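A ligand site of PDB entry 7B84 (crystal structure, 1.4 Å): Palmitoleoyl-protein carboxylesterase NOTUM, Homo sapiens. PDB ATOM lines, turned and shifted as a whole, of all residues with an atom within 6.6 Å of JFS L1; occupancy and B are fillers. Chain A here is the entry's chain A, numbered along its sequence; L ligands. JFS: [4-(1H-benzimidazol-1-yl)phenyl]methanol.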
ATOM      1  N   TRP A  51       8.000  15.468  38.935  1.00  0.00           N
ATOM      2  CA  TRP A  51       7.718  16.683  38.174  1.00  0.00           C
ATOM      3  C   TRP A  51       7.906  17.948  39.011  1.00  0.00           C
ATOM      4  O   TRP A  51       8.831  18.002  39.828  1.00  0.00           O
ATOM      5  CB  TRP A  51       6.374  16.578  37.429  1.00  0.00           C
ATOM      6  CG  TRP A  51       6.408  15.523  36.315  1.00  0.00           C
ATOM      7  CD1 TRP A  51       5.950  14.247  36.394  1.00  0.00           C
ATOM      8  CD2 TRP A  51       6.952  15.672  34.983  1.00  0.00           C
ATOM      9  NE1 TRP A  51       6.149  13.586  35.213  1.00  0.00           N
ATOM     10  CE2 TRP A  51       6.770  14.435  34.328  1.00  0.00           C
ATOM     11  CE3 TRP A  51       7.573  16.717  34.291  1.00  0.00           C
ATOM     12  CZ2 TRP A  51       7.178  14.222  33.016  1.00  0.00           C
ATOM     13  CZ3 TRP A  51       7.976  16.494  32.980  1.00  0.00           C
ATOM     14  CH2 TRP A  51       7.772  15.253  32.356  1.00  0.00           C
ATOM     15  N   TYR A  52       7.079  18.968  38.803  1.00  0.00           N
ATOM     16  CA  TYR A  52       7.206  20.252  39.488  1.00  0.00           C
ATOM     17  C   TYR A  52       5.969  21.084  39.183  1.00  0.00           C
ATOM     18  O   TYR A  52       5.092  20.651  38.429  1.00  0.00           O
ATOM     19  CB  TYR A  52       8.499  20.992  39.096  1.00  0.00           C
ATOM     20  CG  TYR A  52       8.673  21.253  37.611  1.00  0.00           C
ATOM     21  CD1 TYR A  52       8.287  22.465  37.047  1.00  0.00           C
ATOM     22  CD2 TYR A  52       9.239  20.296  36.777  1.00  0.00           C
ATOM     23  CE1 TYR A  52       8.450  22.703  35.684  1.00  0.00           C
ATOM     24  CE2 TYR A  52       9.411  20.531  35.416  1.00  0.00           C
ATOM     25  CZ  TYR A  52       9.012  21.734  34.885  1.00  0.00           C
ATOM     26  OH  TYR A  52       9.176  21.987  33.539  1.00  0.00           O
ATOM     27  N   VAL A 110      12.397  21.129  41.400  1.00  0.00           N
ATOM     28  CA  VAL A 110      13.492  20.347  40.822  1.00  0.00           C
ATOM     29  C   VAL A 110      14.716  20.543  41.733  1.00  0.00           C
ATOM     30  O   VAL A 110      15.867  20.535  41.279  1.00  0.00           O
ATOM     31  CB  VAL A 110      13.730  20.726  39.341  1.00  0.00           C
ATOM     32  CG1 VAL A 110      14.922  19.971  38.704  1.00  0.00           C
ATOM     33  CG2 VAL A 110      12.457  20.576  38.514  1.00  0.00           C
ATOM     34  N   THR A 159      18.064  15.293  38.102  1.00  0.00           N
ATOM     35  CA  THR A 159      18.466  16.650  37.757  1.00  0.00           C
ATOM     36  C   THR A 159      18.911  17.412  38.990  1.00  0.00           C
ATOM     37  O   THR A 159      19.867  18.201  38.935  1.00  0.00           O
ATOM     38  CB  THR A 159      17.315  17.364  37.047  1.00  0.00           C
ATOM     39  OG1 THR A 159      16.805  16.550  35.990  1.00  0.00           O
ATOM     40  CG2 THR A 159      17.781  18.689  36.467  1.00  0.00           C
ATOM     41  N   GLY A 189      17.671  11.906  34.822  1.00  0.00           N
ATOM     42  CA  GLY A 189      17.594  13.351  34.855  1.00  0.00           C
ATOM     43  C   GLY A 189      18.417  14.049  33.782  1.00  0.00           C
ATOM     44  O   GLY A 189      18.727  15.233  33.911  1.00  0.00           O
ATOM     45  N   PHE A 191      18.332  15.178  30.125  1.00  0.00           N
ATOM     46  CA  PHE A 191      17.367  15.459  29.070  1.00  0.00           C
ATOM     47  C   PHE A 191      17.998  16.264  27.926  1.00  0.00           C
ATOM     48  O   PHE A 191      19.033  16.912  28.085  1.00  0.00           O
ATOM     49  CB  PHE A 191      16.149  16.208  29.630  1.00  0.00           C
ATOM     50  CG  PHE A 191      15.394  15.428  30.654  1.00  0.00           C
ATOM     51  CD1 PHE A 191      15.568  15.667  32.001  1.00  0.00           C
ATOM     52  CD2 PHE A 191      14.532  14.415  30.264  1.00  0.00           C
ATOM     53  CE1 PHE A 191      14.881  14.936  32.945  1.00  0.00           C
ATOM     54  CE2 PHE A 191      13.841  13.675  31.209  1.00  0.00           C
ATOM     55  CZ  PHE A 191      14.015  13.935  32.550  1.00  0.00           C
ATOM     56  N   LEU A 192      17.337  16.199  26.770  1.00  0.00           N
ATOM     57  CA  LEU A 192      17.742  16.926  25.575  1.00  0.00           C
ATOM     58  C   LEU A 192      16.706  17.980  25.241  1.00  0.00           C
ATOM     59  O   LEU A 192      15.506  17.686  25.232  1.00  0.00           O
ATOM     60  CB  LEU A 192      17.870  15.976  24.378  1.00  0.00           C
ATOM     61  CG  LEU A 192      18.791  14.760  24.503  1.00  0.00           C
ATOM     62  CD1 LEU A 192      18.736  13.933  23.230  1.00  0.00           C
ATOM     63  CD2 LEU A 192      20.211  15.213  24.791  1.00  0.00           C
ATOM     64  N   ASP A 193      17.154  19.201  24.955  1.00  0.00           N
ATOM     65  CA  ASP A 193      16.243  20.272  24.528  1.00  0.00           C
ATOM     66  C   ASP A 193      16.061  20.225  23.003  1.00  0.00           C
ATOM     67  O   ASP A 193      16.430  21.137  22.263  1.00  0.00           O
ATOM     68  CB  ASP A 193      16.718  21.629  25.029  1.00  0.00           C
ATOM     69  CG  ASP A 193      18.194  21.895  24.749  1.00  0.00           C
ATOM     70  OD1 ASP A 193      18.613  23.071  24.843  1.00  0.00           O
ATOM     71  OD2 ASP A 193      18.944  20.934  24.451  1.00  0.00           O
ATOM     72  N   ASN A 194      15.439  19.130  22.557  1.00  0.00           N
ATOM     73  CA  ASN A 194      15.286  18.839  21.134  1.00  0.00           C
ATOM     74  C   ASN A 194      13.956  19.379  20.611  1.00  0.00           C
ATOM     75  O   ASN A 194      13.122  19.912  21.349  1.00  0.00           O
ATOM     76  CB  ASN A 194      15.400  17.335  20.882  1.00  0.00           C
ATOM     77  CG  ASN A 194      14.281  16.537  21.561  1.00  0.00           C
ATOM     78  OD1 ASN A 194      13.590  17.029  22.448  1.00  0.00           O
ATOM     79  ND2 ASN A 194      14.101  15.292  21.121  1.00  0.00           N
ATOM     80  N   LYS A 195      13.747  19.237  19.303  1.00  0.00           N
ATOM     81  CA  LYS A 195      12.454  19.572  18.723  1.00  0.00           C
ATOM     82  C   LYS A 195      11.437  18.494  19.081  1.00  0.00           C
ATOM     83  O   LYS A 195      11.763  17.312  19.151  1.00  0.00           O
ATOM     84  CB  LYS A 195      12.528  19.714  17.197  1.00  0.00           C
ATOM     85  CG  LYS A 195      12.984  18.464  16.439  1.00  0.00           C
ATOM     86  CD  LYS A 195      12.685  18.578  14.941  1.00  0.00           C
ATOM     87  CE  LYS A 195      13.281  17.401  14.170  1.00  0.00           C
ATOM     88  NZ  LYS A 195      13.554  17.714  12.736  1.00  0.00           N
ATOM     89  N   GLN A 196      10.200  18.923  19.316  1.00  0.00           N
ATOM     90  CA  GLN A 196       9.124  18.019  19.643  1.00  0.00           C
ATOM     91  C   GLN A 196       8.635  17.298  18.391  1.00  0.00           C
ATOM     92  O   GLN A 196       8.821  17.765  17.266  1.00  0.00           O
ATOM     93  CB  GLN A 196       7.978  18.814  20.263  1.00  0.00           C
ATOM     94  CG  GLN A 196       8.302  19.395  21.631  1.00  0.00           C
ATOM     95  CD  GLN A 196       7.222  20.335  22.131  1.00  0.00           C
ATOM     96  OE1 GLN A 196       7.012  21.407  21.563  1.00  0.00           O
ATOM     97  NE2 GLN A 196       6.541  19.940  23.192  1.00  0.00           N
ATOM     98  N   ALA A 209       6.631  26.611  24.023  1.00  0.00           N
ATOM     99  CA  ALA A 209       7.806  25.735  24.004  1.00  0.00           C
ATOM    100  C   ALA A 209       8.073  25.163  25.397  1.00  0.00           C
ATOM    101  O   ALA A 209       7.888  25.845  26.405  1.00  0.00           O
ATOM    102  CB  ALA A 209       9.016  26.489  23.489  1.00  0.00           C
ATOM    103  N   PRO A 210       8.517  23.902  25.445  1.00  0.00           N
ATOM    104  CA  PRO A 210       8.650  23.230  26.754  1.00  0.00           C
ATOM    105  C   PRO A 210       9.689  23.849  27.675  1.00  0.00           C
ATOM    106  O   PRO A 210       9.552  23.748  28.893  1.00  0.00           O
ATOM    107  CB  PRO A 210       8.981  21.781  26.389  1.00  0.00           C
ATOM    108  CG  PRO A 210       9.445  21.804  24.979  1.00  0.00           C
ATOM    109  CD  PRO A 210       8.984  23.068  24.325  1.00  0.00           C
ATOM    110  N   THR A 211      10.739  24.484  27.132  1.00  0.00           N
ATOM    111  CA  THR A 211      11.724  25.137  27.981  1.00  0.00           C
ATOM    112  C   THR A 211      11.178  26.374  28.678  1.00  0.00           C
ATOM    113  O   THR A 211      11.750  26.818  29.680  1.00  0.00           O
ATOM    114  CB  THR A 211      12.990  25.483  27.180  1.00  0.00           C
ATOM    115  OG1 THR A 211      12.642  26.300  26.058  1.00  0.00           O
ATOM    116  CG2 THR A 211      13.694  24.218  26.717  1.00  0.00           C
ATOM    117  N   ALA A 213       8.562  26.573  30.487  1.00  0.00           N
ATOM    118  CA  ALA A 213       8.134  26.217  31.837  1.00  0.00           C
ATOM    119  C   ALA A 213       9.282  26.255  32.840  1.00  0.00           C
ATOM    120  O   ALA A 213       9.066  26.533  34.022  1.00  0.00           O
ATOM    121  CB  ALA A 213       7.450  24.846  31.839  1.00  0.00           C
ATOM    122  N   ILE A 214      10.513  25.975  32.388  1.00  0.00           N
ATOM    123  CA  ILE A 214      11.712  26.011  33.250  1.00  0.00           C
ATOM    124  C   ILE A 214      12.093  27.443  33.566  1.00  0.00           C
ATOM    125  O   ILE A 214      12.148  27.851  34.726  1.00  0.00           O
ATOM    126  CB  ILE A 214      12.898  25.251  32.625  1.00  0.00           C
ATOM    127  CG1 ILE A 214      12.458  23.877  32.135  1.00  0.00           C
ATOM    128  CG2 ILE A 214      14.061  25.206  33.603  1.00  0.00           C
ATOM    129  CD1 ILE A 214      13.560  23.109  31.436  1.00  0.00           C
ATOM    130  N   PHE A 242      19.763  23.288  33.621  1.00  0.00           N
ATOM    131  CA  PHE A 242      18.913  22.145  33.929  1.00  0.00           C
ATOM    132  C   PHE A 242      19.108  21.001  32.941  1.00  0.00           C
ATOM    133  O   PHE A 242      18.490  19.937  33.121  1.00  0.00           O
ATOM    134  CB  PHE A 242      17.435  22.558  33.953  1.00  0.00           C
ATOM    135  CG  PHE A 242      17.029  23.288  35.210  1.00  0.00           C
ATOM    136  CD1 PHE A 242      17.642  24.480  35.561  1.00  0.00           C
ATOM    137  CD2 PHE A 242      16.029  22.781  36.017  1.00  0.00           C
ATOM    138  CE1 PHE A 242      17.271  25.145  36.716  1.00  0.00           C
ATOM    139  CE2 PHE A 242      15.649  23.450  37.169  1.00  0.00           C
ATOM    140  CZ  PHE A 242      16.273  24.635  37.513  1.00  0.00           C
ATOM    141  N   PHE A 243      19.938  21.179  31.927  1.00  0.00           N
ATOM    142  CA  PHE A 243      20.182  20.154  30.919  1.00  0.00           C
ATOM    143  C   PHE A 243      21.561  19.548  31.131  1.00  0.00           C
ATOM    144  O   PHE A 243      22.576  20.252  31.090  1.00  0.00           O
ATOM    145  CB  PHE A 243      19.988  20.731  29.514  1.00  0.00           C
ATOM    146  CG  PHE A 243      18.555  20.990  29.181  1.00  0.00           C
ATOM    147  CD1 PHE A 243      17.946  22.186  29.521  1.00  0.00           C
ATOM    148  CD2 PHE A 243      17.788  20.004  28.584  1.00  0.00           C
ATOM    149  CE1 PHE A 243      16.613  22.406  29.246  1.00  0.00           C
ATOM    150  CE2 PHE A 243      16.453  20.212  28.302  1.00  0.00           C
ATOM    151  CZ  PHE A 243      15.863  21.420  28.631  1.00  0.00           C
ATOM    152  N   ALA A 265       9.775  10.199  30.224  1.00  0.00           N
ATOM    153  CA  ALA A 265       9.522  11.608  30.496  1.00  0.00           C
ATOM    154  C   ALA A 265       9.993  12.485  29.348  1.00  0.00           C
ATOM    155  O   ALA A 265       9.329  13.464  28.986  1.00  0.00           O
ATOM    156  CB  ALA A 265      10.192  12.017  31.809  1.00  0.00           C
ATOM    157  N   GLN A 266      11.146  12.143  28.756  1.00  0.00           N
ATOM    158  CA  GLN A 266      11.622  12.860  27.574  1.00  0.00           C
ATOM    159  C   GLN A 266      10.606  12.756  26.442  1.00  0.00           C
ATOM    160  O   GLN A 266      10.273  13.761  25.803  1.00  0.00           O
ATOM    161  CB  GLN A 266      12.959  12.250  27.136  1.00  0.00           C
ATOM    162  CG  GLN A 266      13.480  12.729  25.781  1.00  0.00           C
ATOM    163  CD  GLN A 266      14.206  14.054  25.874  1.00  0.00           C
ATOM    164  OE1 GLN A 266      15.066  14.247  26.743  1.00  0.00           O
ATOM    165  NE2 GLN A 266      13.888  14.978  24.977  1.00  0.00           N
ATOM    166  N   VAL A 269       7.477  14.895  26.922  1.00  0.00           N
ATOM    167  CA  VAL A 269       7.430  16.342  26.737  1.00  0.00           C
ATOM    168  C   VAL A 269       7.602  16.588  25.235  1.00  0.00           C
ATOM    169  O   VAL A 269       7.221  17.650  24.730  1.00  0.00           O
ATOM    170  CB  VAL A 269       8.498  17.198  27.460  1.00  0.00           C
ATOM    171  CG1 VAL A 269       8.568  17.025  29.027  1.00  0.00           C
ATOM    172  CG2 VAL A 269       9.715  17.644  26.631  1.00  0.00           C
ATOM    173  N   ASP A 270       8.153  15.597  24.515  1.00  0.00           N
ATOM    174  CA  ASP A 270       8.255  15.589  23.051  1.00  0.00           C
ATOM    175  C   ASP A 270       6.928  15.257  22.358  1.00  0.00           C
ATOM    176  O   ASP A 270       6.894  15.249  21.128  1.00  0.00           O
ATOM    177  CB  ASP A 270       9.318  14.587  22.590  1.00  0.00           C
ATOM    178  CG  ASP A 270      10.737  15.097  22.775  1.00  0.00           C
ATOM    179  OD1 ASP A 270      10.939  16.333  22.692  1.00  0.00           O
ATOM    180  OD2 ASP A 270      11.652  14.274  22.987  1.00  0.00           O
HETATM  181  C10 JFS L   1      12.316  19.594  29.087  1.00  0.00           C
HETATM  182  C13 JFS L   1      12.562  19.199  26.358  1.00  0.00           C
HETATM  183  C15 JFS L   1      12.772  18.377  28.615  1.00  0.00           C
HETATM  184  C01 JFS L   1      14.314  19.597  33.971  1.00  0.00           C
HETATM  185  C02 JFS L   1      15.003  19.247  32.806  1.00  0.00           C
HETATM  186  C03 JFS L   1      14.390  19.267  31.578  1.00  0.00           C
HETATM  187  C04 JFS L   1      13.057  19.657  31.535  1.00  0.00           C
HETATM  188  C05 JFS L   1      12.364  20.020  32.696  1.00  0.00           C
HETATM  189  C06 JFS L   1      13.003  19.988  33.932  1.00  0.00           C
HETATM  190  N07 JFS L   1      11.053  20.378  32.371  1.00  0.00           N
HETATM  191  C08 JFS L   1      10.977  20.260  31.074  1.00  0.00           C
HETATM  192  N09 JFS L   1      12.135  19.815  30.494  1.00  0.00           N
HETATM  193  C11 JFS L   1      11.956  20.592  28.214  1.00  0.00           C
HETATM  194  C12 JFS L   1      12.094  20.405  26.853  1.00  0.00           C
HETATM  195  C14 JFS L   1      12.894  18.195  27.240  1.00  0.00           C
HETATM  196  C16 JFS L   1      12.695  18.997  24.875  1.00  0.00           C
HETATM  197  O17 JFS L   1      12.866  20.218  24.168  1.00  0.00           O
HETATM  198  C10 JFS L   2       3.594  16.464  31.852  1.00  0.00           C
HETATM  199  C13 JFS L   2       1.958  14.241  31.558  1.00  0.00           C
HETATM  200  C15 JFS L   2       2.848  16.296  30.705  1.00  0.00           C
HETATM  201  C01 JFS L   2       5.601  20.278  34.864  1.00  0.00           C
HETATM  202  C02 JFS L   2       4.726  19.281  35.292  1.00  0.00           C
HETATM  203  C03 JFS L   2       4.264  18.312  34.417  1.00  0.00           C
HETATM  204  C04 JFS L   2       4.708  18.380  33.107  1.00  0.00           C
HETATM  205  C05 JFS L   2       5.581  19.387  32.664  1.00  0.00           C
HETATM  206  C06 JFS L   2       6.040  20.340  33.565  1.00  0.00           C
HETATM  207  N07 JFS L   2       5.847  19.216  31.318  1.00  0.00           N
HETATM  208  C08 JFS L   2       5.143  18.180  30.937  1.00  0.00           C
HETATM  209  N09 JFS L   2       4.443  17.606  31.977  1.00  0.00           N
HETATM  210  C11 JFS L   2       3.542  15.516  32.850  1.00  0.00           C
HETATM  211  C12 JFS L   2       2.736  14.403  32.701  1.00  0.00           C
HETATM  212  C14 JFS L   2       2.022  15.197  30.569  1.00  0.00           C
HETATM  213  C16 JFS L   2       1.071  13.041  31.392  1.00  0.00           C
HETATM  214  O17 JFS L   2       1.686  11.849  31.867  1.00  0.00           O
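A nitrogen (N07) of JFS L1 is in hydrogen-bond range of the side-chain hydroxyl (OH) of Tyr 52 (2.7 Å). An oxygen (O17) of JFS L1 sits at hydrogen-bond distance from the backbone NH (N) of Asn 194. An oxygen (O17) of JFS L1 sits at hydrogen-bond distance from the backbone carbonyl oxygen (O) of Asn 194 (2.8 Å).
The backbone carbonyl oxygen of Leu 192 sits close to the side-chain amide oxygen of Asn 194, 3.4 Å away. The side-chain carboxylate of Asp 270 lies close to the side-chain amide oxygen of Asn 194 (2.8 Å). The side-chain amide oxygen (OD1) of Asn 194 sits at hydrogen-bond distance from the side-chain amide nitrogen (NE2) of Gln 266 (3.3 Å). The side-chain amide oxygen (OE1) of Gln 266 sits at hydrogen-bond distance from the backbone NH (N) of Leu 192 (3.0 Å). The side-chain amide nitrogen (NE2) of Gln 196 is in hydrogen-bond range of the backbone carbonyl oxygen (O) of Val 269, 2.8 Å away. NE2 of Gln 266 is in hydrogen-bond range of OD2 of Asp 270 (3.1 Å).
Merely in contact with JFS L1: Leu 192 (3.1 Å), Val 269 (3.3 Å), Asp 193 (3.4 Å), Pro 210 (3.4 Å), Ile 214 (3.5 Å), Phe 242 (3.6 Å), Phe 191 (3.7 Å), Asp 270 (3.9 Å) and Phe 243 (3.9 Å). Hydrophobic or aromatic side chains that line JFS L1: Tyr 52, Phe 191, Pro 210, Ile 214, Phe 243 and Val 269. The nearest printed residue that does not touch JFS L1 is Gln 266 (4.1 Å).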
